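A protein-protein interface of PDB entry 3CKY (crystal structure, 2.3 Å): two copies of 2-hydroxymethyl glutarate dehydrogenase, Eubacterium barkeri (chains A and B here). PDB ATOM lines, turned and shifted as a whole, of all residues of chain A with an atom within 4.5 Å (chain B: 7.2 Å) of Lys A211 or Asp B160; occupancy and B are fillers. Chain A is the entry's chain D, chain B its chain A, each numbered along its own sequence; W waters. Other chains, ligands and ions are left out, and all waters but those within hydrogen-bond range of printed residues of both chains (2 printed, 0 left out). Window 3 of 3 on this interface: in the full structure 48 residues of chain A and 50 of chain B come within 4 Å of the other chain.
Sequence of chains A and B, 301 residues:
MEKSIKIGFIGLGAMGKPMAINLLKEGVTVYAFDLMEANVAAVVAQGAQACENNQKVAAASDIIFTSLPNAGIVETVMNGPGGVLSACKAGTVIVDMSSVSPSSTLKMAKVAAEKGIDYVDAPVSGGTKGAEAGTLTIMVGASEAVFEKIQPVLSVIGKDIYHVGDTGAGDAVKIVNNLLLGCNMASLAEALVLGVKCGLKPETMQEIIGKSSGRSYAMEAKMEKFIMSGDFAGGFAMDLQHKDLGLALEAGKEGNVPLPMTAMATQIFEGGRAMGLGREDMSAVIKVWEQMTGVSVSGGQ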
ATOM      1  N   GLU A 207      20.921 -10.788  -0.415  1.00  0.00           N
ATOM      2  CA  GLU A 207      20.562 -10.337  -1.765  1.00  0.00           C
ATOM      3  C   GLU A 207      21.539 -10.861  -2.811  1.00  0.00           C
ATOM      4  O   GLU A 207      21.125 -11.466  -3.803  1.00  0.00           O
ATOM      5  CB  GLU A 207      20.511  -8.807  -1.824  1.00  0.00           C
ATOM      6  CG  GLU A 207      20.571  -8.170  -3.237  1.00  0.00           C
ATOM      7  CD  GLU A 207      19.278  -8.304  -4.054  1.00  0.00           C
ATOM      8  OE1 GLU A 207      18.407  -9.130  -3.679  1.00  0.00           O
ATOM      9  OE2 GLU A 207      19.149  -7.587  -5.086  1.00  0.00           O
ATOM     10  N   ILE A 208      22.830 -10.622  -2.594  1.00  0.00           N
ATOM     11  CA  ILE A 208      23.841 -10.978  -3.594  1.00  0.00           C
ATOM     12  C   ILE A 208      24.040 -12.488  -3.681  1.00  0.00           C
ATOM     13  O   ILE A 208      23.994 -13.043  -4.778  1.00  0.00           O
ATOM     14  CB  ILE A 208      25.207 -10.256  -3.356  1.00  0.00           C
ATOM     15  CG1 ILE A 208      25.111  -8.773  -3.745  1.00  0.00           C
ATOM     16  CG2 ILE A 208      26.299 -10.871  -4.206  1.00  0.00           C
ATOM     17  CD1 ILE A 208      24.114  -7.991  -2.980  1.00  0.00           C
ATOM     18  N   ILE A 209      24.254 -13.145  -2.539  1.00  0.00           N
ATOM     19  CA  ILE A 209      24.555 -14.577  -2.525  1.00  0.00           C
ATOM     20  C   ILE A 209      23.331 -15.391  -2.928  1.00  0.00           C
ATOM     21  O   ILE A 209      23.456 -16.391  -3.644  1.00  0.00           O
ATOM     22  CB  ILE A 209      25.119 -15.042  -1.156  1.00  0.00           C
ATOM     23  CG1 ILE A 209      26.442 -14.313  -0.871  1.00  0.00           C
ATOM     24  CG2 ILE A 209      25.332 -16.556  -1.132  1.00  0.00           C
ATOM     25  CD1 ILE A 209      26.862 -14.331   0.556  1.00  0.00           C
ATOM     26  N   GLY A 210      22.154 -14.947  -2.495  1.00  0.00           N
ATOM     27  CA  GLY A 210      20.894 -15.589  -2.873  1.00  0.00           C
ATOM     28  C   GLY A 210      20.682 -15.633  -4.376  1.00  0.00           C
ATOM     29  O   GLY A 210      19.981 -16.502  -4.878  1.00  0.00           O
ATOM     30  N   LYS A 211      21.290 -14.686  -5.088  1.00  0.00           N
ATOM     31  CA  LYS A 211      21.231 -14.614  -6.557  1.00  0.00           C
ATOM     32  C   LYS A 211      22.456 -15.186  -7.270  1.00  0.00           C
ATOM     33  O   LYS A 211      22.480 -15.194  -8.487  1.00  0.00           O
ATOM     34  CB  LYS A 211      21.122 -13.153  -7.011  1.00  0.00           C
ATOM     35  CG  LYS A 211      19.731 -12.529  -6.980  1.00  0.00           C
ATOM     36  CD  LYS A 211      19.820 -11.016  -7.275  1.00  0.00           C
ATOM     37  CE  LYS A 211      20.242 -10.702  -8.731  1.00  0.00           C
ATOM     38  NZ  LYS A 211      21.176  -9.512  -8.843  1.00  0.00           N
ATOM     39  N   SER A 212      23.469 -15.640  -6.536  1.00  0.00           N
ATOM     40  CA  SER A 212      24.717 -16.096  -7.152  1.00  0.00           C
ATOM     41  C   SER A 212      24.999 -17.555  -6.774  1.00  0.00           C
ATOM     42  O   SER A 212      24.119 -18.257  -6.262  1.00  0.00           O
ATOM     43  CB  SER A 212      25.880 -15.170  -6.754  1.00  0.00           C
ATOM     44  OG  SER A 212      26.996 -15.327  -7.621  1.00  0.00           O
ATOM     45  N   ARG A 215      24.629 -19.840  -3.213  1.00  0.00           N
ATOM     46  CA  ARG A 215      23.306 -20.093  -2.651  1.00  0.00           C
ATOM     47  C   ARG A 215      23.051 -21.577  -2.359  1.00  0.00           C
ATOM     48  O   ARG A 215      23.588 -22.458  -3.021  1.00  0.00           O
ATOM     49  CB  ARG A 215      22.208 -19.534  -3.580  1.00  0.00           C
ATOM     50  CG  ARG A 215      21.702 -20.524  -4.606  1.00  0.00           C
ATOM     51  CD  ARG A 215      20.646 -19.927  -5.474  1.00  0.00           C
ATOM     52  NE  ARG A 215      21.299 -19.145  -6.509  1.00  0.00           N
ATOM     53  CZ  ARG A 215      21.271 -19.410  -7.805  1.00  0.00           C
ATOM     54  NH1 ARG A 215      20.562 -20.431  -8.281  1.00  0.00           N
ATOM     55  NH2 ARG A 215      21.945 -18.621  -8.627  1.00  0.00           N
ATOM     56  N   SER B 125      30.842 -10.283 -11.538  1.00  0.00           N
ATOM     57  CA  SER B 125      30.474 -11.644 -11.919  1.00  0.00           C
ATOM     58  C   SER B 125      29.645 -11.616 -13.203  1.00  0.00           C
ATOM     59  O   SER B 125      29.074 -10.583 -13.556  1.00  0.00           O
ATOM     60  CB  SER B 125      29.721 -12.342 -10.789  1.00  0.00           C
ATOM     61  OG  SER B 125      28.556 -11.634 -10.425  1.00  0.00           O
ATOM     62  N   GLY B 134      27.280  -6.621 -21.638  1.00  0.00           N
ATOM     63  CA  GLY B 134      27.157  -5.487 -20.725  1.00  0.00           C
ATOM     64  C   GLY B 134      26.208  -5.755 -19.565  1.00  0.00           C
ATOM     65  O   GLY B 134      25.579  -4.828 -19.044  1.00  0.00           O
ATOM     66  N   THR B 135      26.110  -7.021 -19.162  1.00  0.00           N
ATOM     67  CA  THR B 135      25.154  -7.447 -18.136  1.00  0.00           C
ATOM     68  C   THR B 135      25.828  -7.928 -16.853  1.00  0.00           C
ATOM     69  O   THR B 135      25.180  -8.547 -16.003  1.00  0.00           O
ATOM     70  CB  THR B 135      24.237  -8.564 -18.676  1.00  0.00           C
ATOM     71  OG1 THR B 135      25.025  -9.704 -19.055  1.00  0.00           O
ATOM     72  CG2 THR B 135      23.451  -8.058 -19.870  1.00  0.00           C
ATOM     73  N   LEU B 136      27.119  -7.624 -16.710  1.00  0.00           N
ATOM     74  CA  LEU B 136      27.888  -7.999 -15.525  1.00  0.00           C
ATOM     75  C   LEU B 136      27.235  -7.512 -14.235  1.00  0.00           C
ATOM     76  O   LEU B 136      26.682  -6.409 -14.188  1.00  0.00           O
ATOM     77  CB  LEU B 136      29.305  -7.409 -15.593  1.00  0.00           C
ATOM     78  CG  LEU B 136      30.284  -8.017 -16.591  1.00  0.00           C
ATOM     79  CD1 LEU B 136      31.554  -7.181 -16.618  1.00  0.00           C
ATOM     80  CD2 LEU B 136      30.587  -9.470 -16.253  1.00  0.00           C
ATOM     81  N   THR B 137      27.309  -8.334 -13.192  1.00  0.00           N
ATOM     82  CA  THR B 137      26.974  -7.881 -11.841  1.00  0.00           C
ATOM     83  C   THR B 137      28.237  -7.316 -11.234  1.00  0.00           C
ATOM     84  O   THR B 137      29.277  -7.963 -11.254  1.00  0.00           O
ATOM     85  CB  THR B 137      26.406  -9.011 -10.973  1.00  0.00           C
ATOM     86  OG1 THR B 137      25.147  -9.416 -11.516  1.00  0.00           O
ATOM     87  CG2 THR B 137      26.201  -8.549  -9.532  1.00  0.00           C
ATOM     88  N   ILE B 138      28.152  -6.094 -10.730  1.00  0.00           N
ATOM     89  CA  ILE B 138      29.311  -5.385 -10.210  1.00  0.00           C
ATOM     90  C   ILE B 138      29.079  -5.027  -8.749  1.00  0.00           C
ATOM     91  O   ILE B 138      28.094  -4.367  -8.415  1.00  0.00           O
ATOM     92  CB  ILE B 138      29.617  -4.122 -11.042  1.00  0.00           C
ATOM     93  CG1 ILE B 138      29.831  -4.509 -12.525  1.00  0.00           C
ATOM     94  CG2 ILE B 138      30.837  -3.386 -10.474  1.00  0.00           C
ATOM     95  CD1 ILE B 138      30.200  -3.353 -13.455  1.00  0.00           C
ATOM     96  N   MET B 139      29.992  -5.478  -7.884  1.00  0.00           N
ATOM     97  CA  MET B 139      29.868  -5.283  -6.448  1.00  0.00           C
ATOM     98  C   MET B 139      30.914  -4.257  -6.000  1.00  0.00           C
ATOM     99  O   MET B 139      32.113  -4.516  -6.071  1.00  0.00           O
ATOM    100  CB  MET B 139      30.052  -6.618  -5.728  1.00  0.00           C
ATOM    101  CG  MET B 139      28.974  -7.678  -6.070  1.00  0.00           C
ATOM    102  SD  MET B 139      29.609  -9.389  -6.256  1.00  0.00           S
ATOM    103  CE  MET B 139      30.655  -9.164  -7.701  1.00  0.00           C
ATOM    104  N   LEU B 154      29.801   2.546 -14.698  1.00  0.00           N
ATOM    105  CA  LEU B 154      29.538   1.155 -14.314  1.00  0.00           C
ATOM    106  C   LEU B 154      28.269   0.614 -14.981  1.00  0.00           C
ATOM    107  O   LEU B 154      28.217  -0.544 -15.390  1.00  0.00           O
ATOM    108  CB  LEU B 154      29.401   1.042 -12.788  1.00  0.00           C
ATOM    109  CG  LEU B 154      30.630   0.688 -11.949  1.00  0.00           C
ATOM    110  CD1 LEU B 154      31.952   1.047 -12.626  1.00  0.00           C
ATOM    111  CD2 LEU B 154      30.516   1.336 -10.571  1.00  0.00           C
ATOM    112  N   GLY B 158      27.934  -2.946 -16.930  1.00  0.00           N
ATOM    113  CA  GLY B 158      27.210  -3.932 -16.123  1.00  0.00           C
ATOM    114  C   GLY B 158      25.724  -3.650 -16.060  1.00  0.00           C
ATOM    115  O   GLY B 158      25.277  -2.586 -16.473  1.00  0.00           O
ATOM    116  N   LYS B 159      24.959  -4.606 -15.543  1.00  0.00           N
ATOM    117  CA  LYS B 159      23.525  -4.426 -15.345  1.00  0.00           C
ATOM    118  C   LYS B 159      23.213  -4.184 -13.858  1.00  0.00           C
ATOM    119  O   LYS B 159      22.824  -3.070 -13.484  1.00  0.00           O
ATOM    120  CB  LYS B 159      22.756  -5.626 -15.908  1.00  0.00           C
ATOM    121  CG  LYS B 159      21.247  -5.598 -15.681  1.00  0.00           C
ATOM    122  CD  LYS B 159      20.538  -6.583 -16.589  1.00  0.00           C
ATOM    123  CE  LYS B 159      19.141  -6.848 -16.113  1.00  0.00           C
ATOM    124  NZ  LYS B 159      18.350  -7.649 -17.079  1.00  0.00           N
ATOM    125  N   ASP B 160      23.379  -5.211 -13.019  1.00  0.00           N
ATOM    126  CA  ASP B 160      23.149  -5.061 -11.576  1.00  0.00           C
ATOM    127  C   ASP B 160      24.390  -4.506 -10.890  1.00  0.00           C
ATOM    128  O   ASP B 160      25.370  -5.229 -10.655  1.00  0.00           O
ATOM    129  CB  ASP B 160      22.746  -6.390 -10.945  1.00  0.00           C
ATOM    130  CG  ASP B 160      21.366  -6.856 -11.386  1.00  0.00           C
ATOM    131  OD1 ASP B 160      20.611  -6.032 -11.933  1.00  0.00           O
ATOM    132  OD2 ASP B 160      21.035  -8.045 -11.178  1.00  0.00           O
ATOM    133  N   ILE B 161      24.347  -3.207 -10.594  1.00  0.00           N
ATOM    134  CA  ILE B 161      25.459  -2.520  -9.943  1.00  0.00           C
ATOM    135  C   ILE B 161      25.121  -2.334  -8.468  1.00  0.00           C
ATOM    136  O   ILE B 161      24.208  -1.578  -8.124  1.00  0.00           O
ATOM    137  CB  ILE B 161      25.725  -1.136 -10.580  1.00  0.00           C
ATOM    138  CG1 ILE B 161      25.828  -1.241 -12.113  1.00  0.00           C
ATOM    139  CG2 ILE B 161      27.001  -0.500  -9.979  1.00  0.00           C
ATOM    140  CD1 ILE B 161      26.813  -2.274 -12.609  1.00  0.00           C
ATOM    141  N   TYR B 162      25.848  -3.029  -7.601  1.00  0.00           N
ATOM    142  CA  TYR B 162      25.598  -2.975  -6.167  1.00  0.00           C
ATOM    143  C   TYR B 162      26.623  -2.110  -5.445  1.00  0.00           C
ATOM    144  O   TYR B 162      27.843  -2.287  -5.620  1.00  0.00           O
ATOM    145  CB  TYR B 162      25.643  -4.369  -5.567  1.00  0.00           C
ATOM    146  CG  TYR B 162      24.503  -5.255  -5.982  1.00  0.00           C
ATOM    147  CD1 TYR B 162      23.302  -5.242  -5.283  1.00  0.00           C
ATOM    148  CD2 TYR B 162      24.631  -6.128  -7.062  1.00  0.00           C
ATOM    149  CE1 TYR B 162      22.255  -6.066  -5.651  1.00  0.00           C
ATOM    150  CE2 TYR B 162      23.589  -6.963  -7.437  1.00  0.00           C
ATOM    151  CZ  TYR B 162      22.403  -6.925  -6.734  1.00  0.00           C
ATOM    152  OH  TYR B 162      21.348  -7.748  -7.090  1.00  0.00           O
ATOM    153  N   ASN B 177      30.760 -15.293  -1.331  1.00  0.00           N
ATOM    154  CA  ASN B 177      30.001 -16.116  -2.254  1.00  0.00           C
ATOM    155  C   ASN B 177      30.789 -17.327  -2.741  1.00  0.00           C
ATOM    156  O   ASN B 177      30.285 -18.443  -2.715  1.00  0.00           O
ATOM    157  CB  ASN B 177      29.522 -15.304  -3.460  1.00  0.00           C
ATOM    158  CG  ASN B 177      28.770 -16.169  -4.477  1.00  0.00           C
ATOM    159  OD1 ASN B 177      27.624 -16.538  -4.257  1.00  0.00           O
ATOM    160  ND2 ASN B 177      29.435 -16.511  -5.588  1.00  0.00           N
ATOM    161  N   TYR B 217      23.198 -24.498  -5.307  1.00  0.00           N
ATOM    162  CA  TYR B 217      23.551 -24.160  -6.671  1.00  0.00           C
ATOM    163  C   TYR B 217      24.727 -25.021  -7.165  1.00  0.00           C
ATOM    164  O   TYR B 217      24.724 -25.481  -8.293  1.00  0.00           O
ATOM    165  CB  TYR B 217      23.870 -22.669  -6.804  1.00  0.00           C
ATOM    166  CG  TYR B 217      24.353 -22.339  -8.171  1.00  0.00           C
ATOM    167  CD1 TYR B 217      23.459 -22.132  -9.210  1.00  0.00           C
ATOM    168  CD2 TYR B 217      25.704 -22.296  -8.453  1.00  0.00           C
ATOM    169  CE1 TYR B 217      23.906 -21.857 -10.502  1.00  0.00           C
ATOM    170  CE2 TYR B 217      26.157 -22.022  -9.728  1.00  0.00           C
ATOM    171  CZ  TYR B 217      25.252 -21.800 -10.736  1.00  0.00           C
ATOM    172  OH  TYR B 217      25.707 -21.536 -11.988  1.00  0.00           O
HETATM  173  O   HOH W   1      26.004 -23.300  -3.754  1.00  0.00           O
HETATM  174  O   HOH W   2      29.002 -13.622  -6.922  1.00  0.00           O
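NZ of Lys A211 sits at hydrogen-bond distance from OH of Tyr B162.
NZ of Lys A211 lies within salt-bridge range of OD2 of Asp B160, 2.8 Å away.
The side-chain hydroxyl (OH) of Tyr B162 lies within hydrogen-bond range of the side-chain carboxylate (OE2) of Glu A207.
The backbone NH (N) of Tyr B217 sits at hydrogen-bond distance from the backbone carbonyl oxygen (O) of Arg A215.
The side-chain hydroxyl (OG) of Ser A212 lies within hydrogen-bond range of the side-chain amide nitrogen (ND2) of Asn B177 (3.4 Å).
The backbone NH (N) of Tyr B162 sits at hydrogen-bond distance from the backbone carbonyl oxygen (O) of Ile B138, at 2.7 Å.
O of Ser A212 is in hydrogen-bond range of NE of Arg A215, at 3.0 Å.
The guanidinium group (NE) of Arg A215 is in hydrogen-bond range of the backbone carbonyl oxygen (O) of Gly A210, at 3.4 Å.
The guanidinium group of Arg A215 is in hydrogen-bond range of the backbone carbonyl oxygen of Lys A211 (3.5 Å).
The backbone carbonyl oxygen (O) of Asp B160 sits at hydrogen-bond distance from the backbone NH (N) of Ile B138, 2.9 Å away.
Among the printed residues, pairs that only touch across the chains: Ile A208 with Tyr B162 and Ile A209 with Asn B177.
Printed residues of chain B within 4 Å of Ile A209: Asn B177.
Lys A211 touches just these residues of chain B: Asp B160 (2.8 Å) and Tyr B162 (2.5 Å).
Printed residues of chain B within 4 Å of Arg A215: Tyr B217.
Asp B160 touches just one residue of chain A: Lys A211 (2.8 Å).
Hydrophobic or aromatic side chains of chain A within 4 Å of the printed part of chain B: Ile A208 and Ile A209.
Among the printed residues, Asp or Glu carboxylates within 4 Å of a Lys or Arg side-chain nitrogen of the other chain: Lys A211 with Asp B160.
No position is printed for both chains.
Water W1 lies within hydrogen-bond range of the backbone carbonyl oxygen (O) of Arg A215 and the backbone NH (N) of Tyr B217.
Water W2 bridges the side-chain hydroxyl (OG) of Ser A212 (2.7 Å) and the side-chain amide nitrogen (ND2) of Asn B177 (3.2 Å).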
